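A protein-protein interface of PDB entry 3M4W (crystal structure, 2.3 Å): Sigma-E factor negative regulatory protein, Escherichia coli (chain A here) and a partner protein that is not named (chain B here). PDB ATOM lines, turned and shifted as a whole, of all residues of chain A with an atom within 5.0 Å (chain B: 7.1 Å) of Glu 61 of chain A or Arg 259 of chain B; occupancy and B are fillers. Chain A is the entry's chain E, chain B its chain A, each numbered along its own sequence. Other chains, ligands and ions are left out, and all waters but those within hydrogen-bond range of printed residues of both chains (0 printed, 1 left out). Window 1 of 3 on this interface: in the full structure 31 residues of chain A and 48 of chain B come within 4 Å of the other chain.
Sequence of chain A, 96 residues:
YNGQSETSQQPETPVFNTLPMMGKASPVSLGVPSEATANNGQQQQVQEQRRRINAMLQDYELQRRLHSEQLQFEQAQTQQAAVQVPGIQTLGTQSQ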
ATOM      1  N   VAL A  28      20.503  -8.449  34.287  1.00  0.00           N
ATOM      2  CA  VAL A  28      19.453  -9.351  33.824  1.00  0.00           C
ATOM      3  C   VAL A  28      18.099  -8.637  33.833  1.00  0.00           C
ATOM      4  O   VAL A  28      17.652  -8.136  34.868  1.00  0.00           O
ATOM      5  CB  VAL A  28      19.372 -10.621  34.703  1.00  0.00           C
ATOM      6  CG1 VAL A  28      18.970 -10.259  36.125  1.00  0.00           C
ATOM      7  CG2 VAL A  28      18.389 -11.596  34.098  1.00  0.00           C
ATOM      8  N   LEU A  57      13.521 -15.167  25.459  1.00  0.00           N
ATOM      9  CA  LEU A  57      14.968 -15.228  25.527  1.00  0.00           C
ATOM     10  C   LEU A  57      15.467 -14.675  26.863  1.00  0.00           C
ATOM     11  O   LEU A  57      16.236 -15.327  27.569  1.00  0.00           O
ATOM     12  CB  LEU A  57      15.573 -14.426  24.372  1.00  0.00           C
ATOM     13  CG  LEU A  57      17.028 -14.720  23.999  1.00  0.00           C
ATOM     14  CD1 LEU A  57      17.149 -16.170  23.538  1.00  0.00           C
ATOM     15  CD2 LEU A  57      17.482 -13.768  22.898  1.00  0.00           C
ATOM     16  N   GLN A  58      15.024 -13.472  27.214  1.00  0.00           N
ATOM     17  CA  GLN A  58      15.457 -12.869  28.462  1.00  0.00           C
ATOM     18  C   GLN A  58      14.788 -13.495  29.686  1.00  0.00           C
ATOM     19  O   GLN A  58      15.171 -13.218  30.819  1.00  0.00           O
ATOM     20  CB  GLN A  58      15.220 -11.359  28.437  1.00  0.00           C
ATOM     21  CG  GLN A  58      13.775 -10.959  28.333  1.00  0.00           C
ATOM     22  CD  GLN A  58      13.545  -9.546  28.812  1.00  0.00           C
ATOM     23  OE1 GLN A  58      13.788  -8.577  28.090  1.00  0.00           O
ATOM     24  NE2 GLN A  58      13.084  -9.418  30.050  1.00  0.00           N
ATOM     25  N   ASP A  59      13.789 -14.338  29.469  1.00  0.00           N
ATOM     26  CA  ASP A  59      13.147 -15.004  30.595  1.00  0.00           C
ATOM     27  C   ASP A  59      13.978 -16.242  30.903  1.00  0.00           C
ATOM     28  O   ASP A  59      14.051 -16.701  32.048  1.00  0.00           O
ATOM     29  CB  ASP A  59      11.723 -15.419  30.254  1.00  0.00           C
ATOM     30  CG  ASP A  59      11.035 -16.106  31.414  1.00  0.00           C
ATOM     31  OD1 ASP A  59      10.886 -15.474  32.483  1.00  0.00           O
ATOM     32  OD2 ASP A  59      10.654 -17.281  31.263  1.00  0.00           O
ATOM     33  N   TYR A  60      14.596 -16.784  29.857  1.00  0.00           N
ATOM     34  CA  TYR A  60      15.470 -17.946  29.985  1.00  0.00           C
ATOM     35  C   TYR A  60      16.674 -17.511  30.823  1.00  0.00           C
ATOM     36  O   TYR A  60      17.112 -18.225  31.721  1.00  0.00           O
ATOM     37  CB  TYR A  60      15.942 -18.404  28.597  1.00  0.00           C
ATOM     38  CG  TYR A  60      17.247 -19.175  28.596  1.00  0.00           C
ATOM     39  CD1 TYR A  60      17.321 -20.463  29.101  1.00  0.00           C
ATOM     40  CD2 TYR A  60      18.413 -18.598  28.107  1.00  0.00           C
ATOM     41  CE1 TYR A  60      18.522 -21.159  29.120  1.00  0.00           C
ATOM     42  CE2 TYR A  60      19.624 -19.285  28.124  1.00  0.00           C
ATOM     43  CZ  TYR A  60      19.672 -20.561  28.631  1.00  0.00           C
ATOM     44  OH  TYR A  60      20.875 -21.232  28.673  1.00  0.00           O
ATOM     45  N   GLU A  61      17.194 -16.322  30.524  1.00  0.00           N
ATOM     46  CA  GLU A  61      18.348 -15.803  31.237  1.00  0.00           C
ATOM     47  C   GLU A  61      17.988 -15.551  32.696  1.00  0.00           C
ATOM     48  O   GLU A  61      18.702 -15.989  33.596  1.00  0.00           O
ATOM     49  CB  GLU A  61      18.839 -14.502  30.591  1.00  0.00           C
ATOM     50  CG  GLU A  61      19.511 -14.660  29.222  1.00  0.00           C
ATOM     51  CD  GLU A  61      20.646 -15.673  29.230  1.00  0.00           C
ATOM     52  OE1 GLU A  61      21.345 -15.788  30.259  1.00  0.00           O
ATOM     53  OE2 GLU A  61      20.847 -16.352  28.202  1.00  0.00           O
ATOM     54  N   LEU A  62      16.877 -14.845  32.914  1.00  0.00           N
ATOM     55  CA  LEU A  62      16.387 -14.518  34.256  1.00  0.00           C
ATOM     56  C   LEU A  62      16.324 -15.794  35.084  1.00  0.00           C
ATOM     57  O   LEU A  62      16.735 -15.818  36.239  1.00  0.00           O
ATOM     58  CB  LEU A  62      14.985 -13.900  34.171  1.00  0.00           C
ATOM     59  CG  LEU A  62      14.532 -12.790  35.136  1.00  0.00           C
ATOM     60  CD1 LEU A  62      13.024 -12.930  35.339  1.00  0.00           C
ATOM     61  CD2 LEU A  62      15.242 -12.874  36.487  1.00  0.00           C
ATOM     62  N   GLN A  63      15.817 -16.855  34.465  1.00  0.00           N
ATOM     63  CA  GLN A  63      15.674 -18.174  35.088  1.00  0.00           C
ATOM     64  C   GLN A  63      17.024 -18.790  35.450  1.00  0.00           C
ATOM     65  O   GLN A  63      17.199 -19.323  36.554  1.00  0.00           O
ATOM     66  CB  GLN A  63      14.955 -19.122  34.127  1.00  0.00           C
ATOM     67  CG  GLN A  63      13.787 -19.894  34.703  1.00  0.00           C
ATOM     68  CD  GLN A  63      12.450 -19.294  34.314  1.00  0.00           C
ATOM     69  OE1 GLN A  63      11.436 -19.991  34.277  1.00  0.00           O
ATOM     70  NE2 GLN A  63      12.440 -17.992  34.027  1.00  0.00           N
ATOM     71  N   ARG A  64      17.967 -18.737  34.506  1.00  0.00           N
ATOM     72  CA  ARG A  64      19.311 -19.290  34.706  1.00  0.00           C
ATOM     73  C   ARG A  64      19.960 -18.782  35.981  1.00  0.00           C
ATOM     74  O   ARG A  64      20.635 -19.528  36.688  1.00  0.00           O
ATOM     75  CB  ARG A  64      20.236 -18.923  33.539  1.00  0.00           C
ATOM     76  CG  ARG A  64      20.032 -19.717  32.277  1.00  0.00           C
ATOM     77  CD  ARG A  64      21.350 -19.836  31.523  1.00  0.00           C
ATOM     78  NE  ARG A  64      21.891 -18.544  31.097  1.00  0.00           N
ATOM     79  CZ  ARG A  64      23.178 -18.231  31.178  1.00  0.00           C
ATOM     80  NH1 ARG A  64      24.032 -19.119  31.673  1.00  0.00           N
ATOM     81  NH2 ARG A  64      23.609 -17.042  30.778  1.00  0.00           N
ATOM     82  N   ARG A  65      19.767 -17.497  36.245  1.00  0.00           N
ATOM     83  CA  ARG A  65      20.347 -16.846  37.412  1.00  0.00           C
ATOM     84  C   ARG A  65      19.516 -17.045  38.685  1.00  0.00           C
ATOM     85  O   ARG A  65      20.059 -17.072  39.793  1.00  0.00           O
ATOM     86  CB  ARG A  65      20.540 -15.359  37.103  1.00  0.00           C
ATOM     87  CG  ARG A  65      21.410 -15.135  35.873  1.00  0.00           C
ATOM     88  CD  ARG A  65      21.436 -13.682  35.439  1.00  0.00           C
ATOM     89  NE  ARG A  65      22.508 -13.401  34.478  1.00  0.00           N
ATOM     90  CZ  ARG A  65      22.603 -13.931  33.259  1.00  0.00           C
ATOM     91  NH1 ARG A  65      21.686 -14.786  32.824  1.00  0.00           N
ATOM     92  NH2 ARG A  65      23.621 -13.599  32.469  1.00  0.00           N
ATOM     93  N   VAL B  85      26.497 -15.565  37.182  1.00  0.00           N
ATOM     94  CA  VAL B  85      26.376 -16.267  35.912  1.00  0.00           C
ATOM     95  C   VAL B  85      27.006 -15.437  34.799  1.00  0.00           C
ATOM     96  O   VAL B  85      26.839 -14.217  34.756  1.00  0.00           O
ATOM     97  CB  VAL B  85      24.901 -16.551  35.551  1.00  0.00           C
ATOM     98  CG1 VAL B  85      24.836 -17.494  34.352  1.00  0.00           C
ATOM     99  CG2 VAL B  85      24.178 -17.167  36.741  1.00  0.00           C
ATOM    100  N   ASP B  86      27.742 -16.115  33.913  1.00  0.00           N
ATOM    101  CA  ASP B  86      28.427 -15.466  32.786  1.00  0.00           C
ATOM    102  C   ASP B  86      29.653 -14.692  33.217  1.00  0.00           C
ATOM    103  O   ASP B  86      30.157 -13.889  32.441  1.00  0.00           O
ATOM    104  CB  ASP B  86      27.506 -14.492  32.041  1.00  0.00           C
ATOM    105  CG  ASP B  86      26.590 -15.178  31.051  1.00  0.00           C
ATOM    106  OD1 ASP B  86      26.594 -16.424  30.996  1.00  0.00           O
ATOM    107  OD2 ASP B  86      25.860 -14.459  30.332  1.00  0.00           O
ATOM    108  N   TYR B 131      26.593 -29.368  22.913  1.00  0.00           N
ATOM    109  CA  TYR B 131      27.791 -28.614  22.542  1.00  0.00           C
ATOM    110  C   TYR B 131      28.875 -29.158  23.447  1.00  0.00           C
ATOM    111  O   TYR B 131      28.578 -29.676  24.504  1.00  0.00           O
ATOM    112  CB  TYR B 131      27.623 -27.123  22.851  1.00  0.00           C
ATOM    113  CG  TYR B 131      26.601 -26.421  22.002  1.00  0.00           C
ATOM    114  CD1 TYR B 131      26.555 -26.633  20.621  1.00  0.00           C
ATOM    115  CD2 TYR B 131      25.713 -25.511  22.561  1.00  0.00           C
ATOM    116  CE1 TYR B 131      25.666 -25.952  19.820  1.00  0.00           C
ATOM    117  CE2 TYR B 131      24.804 -24.815  21.752  1.00  0.00           C
ATOM    118  CZ  TYR B 131      24.795 -25.039  20.386  1.00  0.00           C
ATOM    119  OH  TYR B 131      23.970 -24.319  19.559  1.00  0.00           O
ATOM    120  N   LEU B 149      33.865 -23.067  23.815  1.00  0.00           N
ATOM    121  CA  LEU B 149      32.562 -23.744  23.699  1.00  0.00           C
ATOM    122  C   LEU B 149      32.449 -24.096  22.205  1.00  0.00           C
ATOM    123  O   LEU B 149      32.426 -23.209  21.353  1.00  0.00           O
ATOM    124  CB  LEU B 149      31.392 -22.805  24.080  1.00  0.00           C
ATOM    125  CG  LEU B 149      29.968 -23.362  23.856  1.00  0.00           C
ATOM    126  CD1 LEU B 149      29.780 -24.591  24.741  1.00  0.00           C
ATOM    127  CD2 LEU B 149      28.902 -22.310  24.193  1.00  0.00           C
ATOM    128  N   LEU B 157      31.880 -21.462  19.240  1.00  0.00           N
ATOM    129  CA  LEU B 157      30.763 -20.562  19.464  1.00  0.00           C
ATOM    130  C   LEU B 157      31.233 -19.433  20.350  1.00  0.00           C
ATOM    131  O   LEU B 157      30.854 -18.281  20.158  1.00  0.00           O
ATOM    132  CB  LEU B 157      29.613 -21.310  20.152  1.00  0.00           C
ATOM    133  CG  LEU B 157      28.981 -22.422  19.295  1.00  0.00           C
ATOM    134  CD1 LEU B 157      28.038 -23.282  20.155  1.00  0.00           C
ATOM    135  CD2 LEU B 157      28.223 -21.789  18.106  1.00  0.00           C
ATOM    136  N   LEU B 230      11.989 -25.393  32.968  1.00  0.00           N
ATOM    137  CA  LEU B 230      13.445 -25.276  32.897  1.00  0.00           C
ATOM    138  C   LEU B 230      14.193 -26.569  33.192  1.00  0.00           C
ATOM    139  O   LEU B 230      13.887 -27.271  34.160  1.00  0.00           O
ATOM    140  CB  LEU B 230      13.915 -24.196  33.878  1.00  0.00           C
ATOM    141  CG  LEU B 230      15.355 -23.686  33.758  1.00  0.00           C
ATOM    142  CD1 LEU B 230      15.506 -22.918  32.451  1.00  0.00           C
ATOM    143  CD2 LEU B 230      15.691 -22.782  34.947  1.00  0.00           C
ATOM    144  N   LEU B 254      15.984 -20.100  15.284  1.00  0.00           N
ATOM    145  CA  LEU B 254      16.904 -18.974  15.372  1.00  0.00           C
ATOM    146  C   LEU B 254      18.103 -19.380  16.223  1.00  0.00           C
ATOM    147  O   LEU B 254      17.990 -20.217  17.122  1.00  0.00           O
ATOM    148  CB  LEU B 254      16.208 -17.770  16.009  1.00  0.00           C
ATOM    149  CG  LEU B 254      17.118 -16.597  16.389  1.00  0.00           C
ATOM    150  CD1 LEU B 254      17.682 -15.955  15.133  1.00  0.00           C
ATOM    151  CD2 LEU B 254      16.333 -15.579  17.207  1.00  0.00           C
ATOM    152  N   ARG B 255      19.252 -18.782  15.946  1.00  0.00           N
ATOM    153  CA  ARG B 255      20.458 -19.098  16.700  1.00  0.00           C
ATOM    154  C   ARG B 255      21.234 -17.831  17.029  1.00  0.00           C
ATOM    155  O   ARG B 255      21.722 -17.159  16.129  1.00  0.00           O
ATOM    156  CB  ARG B 255      21.344 -20.038  15.888  1.00  0.00           C
ATOM    157  CG  ARG B 255      22.275 -20.877  16.724  1.00  0.00           C
ATOM    158  CD  ARG B 255      23.125 -21.768  15.848  1.00  0.00           C
ATOM    159  NE  ARG B 255      23.761 -22.841  16.606  1.00  0.00           N
ATOM    160  CZ  ARG B 255      24.697 -23.638  16.106  1.00  0.00           C
ATOM    161  NH1 ARG B 255      25.105 -23.474  14.854  1.00  0.00           N
ATOM    162  NH2 ARG B 255      25.211 -24.609  16.851  1.00  0.00           N
ATOM    163  N   THR B 256      21.338 -17.510  18.317  1.00  0.00           N
ATOM    164  CA  THR B 256      22.071 -16.324  18.760  1.00  0.00           C
ATOM    165  C   THR B 256      23.351 -16.755  19.484  1.00  0.00           C
ATOM    166  O   THR B 256      23.444 -16.670  20.712  1.00  0.00           O
ATOM    167  CB  THR B 256      21.235 -15.456  19.732  1.00  0.00           C
ATOM    168  OG1 THR B 256      19.929 -15.227  19.185  1.00  0.00           O
ATOM    169  CG2 THR B 256      21.918 -14.116  19.956  1.00  0.00           C
ATOM    170  N   GLY B 257      24.335 -17.215  18.717  1.00  0.00           N
ATOM    171  CA  GLY B 257      25.578 -17.659  19.312  1.00  0.00           C
ATOM    172  C   GLY B 257      25.393 -19.030  19.924  1.00  0.00           C
ATOM    173  O   GLY B 257      25.311 -20.027  19.212  1.00  0.00           O
ATOM    174  N   ARG B 258      25.311 -19.087  21.248  1.00  0.00           N
ATOM    175  CA  ARG B 258      25.131 -20.361  21.928  1.00  0.00           C
ATOM    176  C   ARG B 258      23.678 -20.616  22.278  1.00  0.00           C
ATOM    177  O   ARG B 258      23.310 -21.746  22.579  1.00  0.00           O
ATOM    178  CB  ARG B 258      25.965 -20.404  23.207  1.00  0.00           C
ATOM    179  CG  ARG B 258      25.610 -19.340  24.239  1.00  0.00           C
ATOM    180  CD  ARG B 258      26.840 -19.012  25.065  1.00  0.00           C
ATOM    181  NE  ARG B 258      26.662 -19.264  26.491  1.00  0.00           N
ATOM    182  CZ  ARG B 258      26.431 -18.312  27.389  1.00  0.00           C
ATOM    183  NH1 ARG B 258      26.347 -17.043  27.006  1.00  0.00           N
ATOM    184  NH2 ARG B 258      26.294 -18.624  28.668  1.00  0.00           N
ATOM    185  N   ARG B 259      22.857 -19.571  22.240  1.00  0.00           N
ATOM    186  CA  ARG B 259      21.452 -19.723  22.582  1.00  0.00           C
ATOM    187  C   ARG B 259      20.583 -20.028  21.374  1.00  0.00           C
ATOM    188  O   ARG B 259      20.589 -19.308  20.375  1.00  0.00           O
ATOM    189  CB  ARG B 259      20.938 -18.474  23.297  1.00  0.00           C
ATOM    190  CG  ARG B 259      21.688 -18.167  24.573  1.00  0.00           C
ATOM    191  CD  ARG B 259      21.037 -17.022  25.312  1.00  0.00           C
ATOM    192  NE  ARG B 259      21.015 -15.792  24.522  1.00  0.00           N
ATOM    193  CZ  ARG B 259      20.390 -14.679  24.898  1.00  0.00           C
ATOM    194  NH1 ARG B 259      19.732 -14.638  26.052  1.00  0.00           N
ATOM    195  NH2 ARG B 259      20.429 -13.602  24.124  1.00  0.00           N
ATOM    196  N   THR B 260      19.836 -21.116  21.483  1.00  0.00           N
ATOM    197  CA  THR B 260      18.955 -21.554  20.427  1.00  0.00           C
ATOM    198  C   THR B 260      17.503 -21.242  20.769  1.00  0.00           C
ATOM    199  O   THR B 260      17.115 -21.181  21.942  1.00  0.00           O
ATOM    200  CB  THR B 260      19.082 -23.073  20.208  1.00  0.00           C
ATOM    201  OG1 THR B 260      20.420 -23.392  19.803  1.00  0.00           O
ATOM    202  CG2 THR B 260      18.090 -23.543  19.157  1.00  0.00           C
ATOM    203  N   VAL B 261      16.708 -21.036  19.730  1.00  0.00           N
ATOM    204  CA  VAL B 261      15.288 -20.776  19.884  1.00  0.00           C
ATOM    205  C   VAL B 261      14.586 -21.552  18.783  1.00  0.00           C
ATOM    206  O   VAL B 261      14.684 -21.214  17.604  1.00  0.00           O
ATOM    207  CB  VAL B 261      14.957 -19.279  19.751  1.00  0.00           C
ATOM    208  CG1 VAL B 261      13.446 -19.077  19.774  1.00  0.00           C
ATOM    209  CG2 VAL B 261      15.590 -18.513  20.892  1.00  0.00           C
ATOM    210  N   VAL B 274      14.223 -22.937  24.327  1.00  0.00           N
ATOM    211  CA  VAL B 274      15.197 -21.854  24.415  1.00  0.00           C
ATOM    212  C   VAL B 274      16.380 -22.234  25.301  1.00  0.00           C
ATOM    213  O   VAL B 274      16.206 -22.590  26.467  1.00  0.00           O
ATOM    214  CB  VAL B 274      14.549 -20.568  24.984  1.00  0.00           C
ATOM    215  CG1 VAL B 274      15.592 -19.476  25.123  1.00  0.00           C
ATOM    216  CG2 VAL B 274      13.421 -20.101  24.069  1.00  0.00           C
ATOM    217  N   GLY B 275      17.588 -22.158  24.759  1.00  0.00           N
ATOM    218  CA  GLY B 275      18.738 -22.510  25.568  1.00  0.00           C
ATOM    219  C   GLY B 275      20.004 -22.922  24.847  1.00  0.00           C
ATOM    220  O   GLY B 275      20.150 -22.731  23.639  1.00  0.00           O
ATOM    221  N   GLU B 276      20.916 -23.512  25.611  1.00  0.00           N
ATOM    222  CA  GLU B 276      22.213 -23.940  25.115  1.00  0.00           C
ATOM    223  C   GLU B 276      22.194 -25.330  24.495  1.00  0.00           C
ATOM    224  O   GLU B 276      22.781 -26.260  25.040  1.00  0.00           O
ATOM    225  CB  GLU B 276      23.216 -23.900  26.267  1.00  0.00           C
ATOM    226  CG  GLU B 276      23.294 -22.542  26.970  1.00  0.00           C
ATOM    227  CD  GLU B 276      23.922 -22.631  28.356  1.00  0.00           C
ATOM    228  OE1 GLU B 276      23.271 -23.202  29.259  1.00  0.00           O
ATOM    229  OE2 GLU B 276      25.064 -22.139  28.540  1.00  0.00           O
ATOM    230  N   LEU B 277      21.537 -25.468  23.348  1.00  0.00           N
ATOM    231  CA  LEU B 277      21.443 -26.770  22.684  1.00  0.00           C
ATOM    232  C   LEU B 277      21.559 -26.702  21.169  1.00  0.00           C
ATOM    233  O   LEU B 277      21.179 -25.719  20.543  1.00  0.00           O
ATOM    234  CB  LEU B 277      20.089 -27.442  22.987  1.00  0.00           C
ATOM    235  CG  LEU B 277      19.662 -27.988  24.354  1.00  0.00           C
ATOM    236  CD1 LEU B 277      18.203 -28.417  24.281  1.00  0.00           C
ATOM    237  CD2 LEU B 277      20.532 -29.160  24.757  1.00  0.00           C
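The guanidinium group (NH2) of Arg 65 of chain A is in salt-bridge range of the side-chain carboxylate (OD2) of Asp 86 of chain B (3.2 Å). The guanidinium group (NH2) of Arg 64 of chain A is in salt-bridge range of the side-chain carboxylate (OD1) of Asp 86 of chain B (3.1 Å). The side-chain carboxylate of Glu 276 of chain B is in hydrogen-bond range of the side-chain hydroxyl of Tyr 60 of chain A, at 3.2 Å. The side-chain carboxylate of Glu 61 of chain A lies within salt-bridge range of the guanidinium group of Arg 259 of chain B (3.0 Å).
The side-chain carboxylate (OE2) of Glu 276 of chain B is in salt-bridge range of the guanidinium group (NH2) of Arg 258 of chain B. OE1 of Glu 61 of chain A lies within salt-bridge range of NH2 of Arg 64 of chain A, 2.6 Å away. The backbone carbonyl oxygen (O) of Val 261 of chain B sits at hydrogen-bond distance from the backbone NH (N) of Leu 254 of chain B (2.9 Å). OE1 of Glu 61 of chain A lies within salt-bridge range of NH1 of Arg 65 of chain A (2.8 Å). O of Asp 59 of chain A sits at hydrogen-bond distance from NE2 of Gln 63 of chain A. NH2 of Arg 258 of chain B is in salt-bridge range of OD1 of Asp 86 of chain B, 3.2 Å away.
NH2 of Arg 259 of chain B touches CD2 of Leu 57 of chain A, at 3.2 Å. Leu 57 of chain A touches Val 261 of chain B. Val 274 of chain B touches Leu 57 of chain A (CG1 to CD1, 3.98 Å). Arg 259 of chain B touches Tyr 60 of chain A. O of Val 274 of chain B touches CD1 of Tyr 60 of chain A, 3.6 Å away. CZ of Tyr 60 of chain A touches CA of Gly 275 of chain B, at 3.7 Å. CG of Gln 63 of chain A touches CD2 of Leu 230 of chain B, at 3.5 Å. Arg 64 of chain A touches Val 85 of chain B. NH2 of Arg 64 of chain A touches NH2 of Arg 258 of chain B, 3.8 Å away. Val 85 of chain B touches Arg 65 of chain A.
Glu 61 of chain A touches one residue of chain B. Arg 259 of chain B touches three residues of chain A. Printed residues of chain B within 4 Å of Arg 64 of chain A: Val 85, Asp 86 and Arg 258. Of the printed residues of chain A, Glu 276 of chain B touches Tyr 60. Printed residues of chain A within 4 Å of Gly 275 of chain B: Tyr 60. Printed residues of chain A within 4 Å of Leu 230 of chain B: Gln 63. Leu 277 of chain B touches none of the printed residues of chain A. The nearest printed residue of chain A that does not touch Arg 259 of chain B is Gln 58 of chain A (5.0 Å). The nearest printed residue of chain A that does not touch Leu 230 of chain B is Tyr 60 of chain A (4.5 Å).
Of the 18 printed residues of chain B, 9 touch a printed residue of chain A. Hydrophobic or aromatic side chains of chain B within 4 Å of the printed part of chain A: Val 85, Leu 230, Val 261 and Val 274. Along chain B the printed residues that touch a printed residue of chain A span positions 85 to 276. Among the printed residues, Asp or Glu carboxylates within 4 Å of a Lys or Arg side-chain nitrogen of the other chain: Glu 61 of chain A with Arg 259 of chain B, Arg 64 of chain A with Asp 86 of chain B and Arg 65 of chain A with Asp 86 of chain B.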
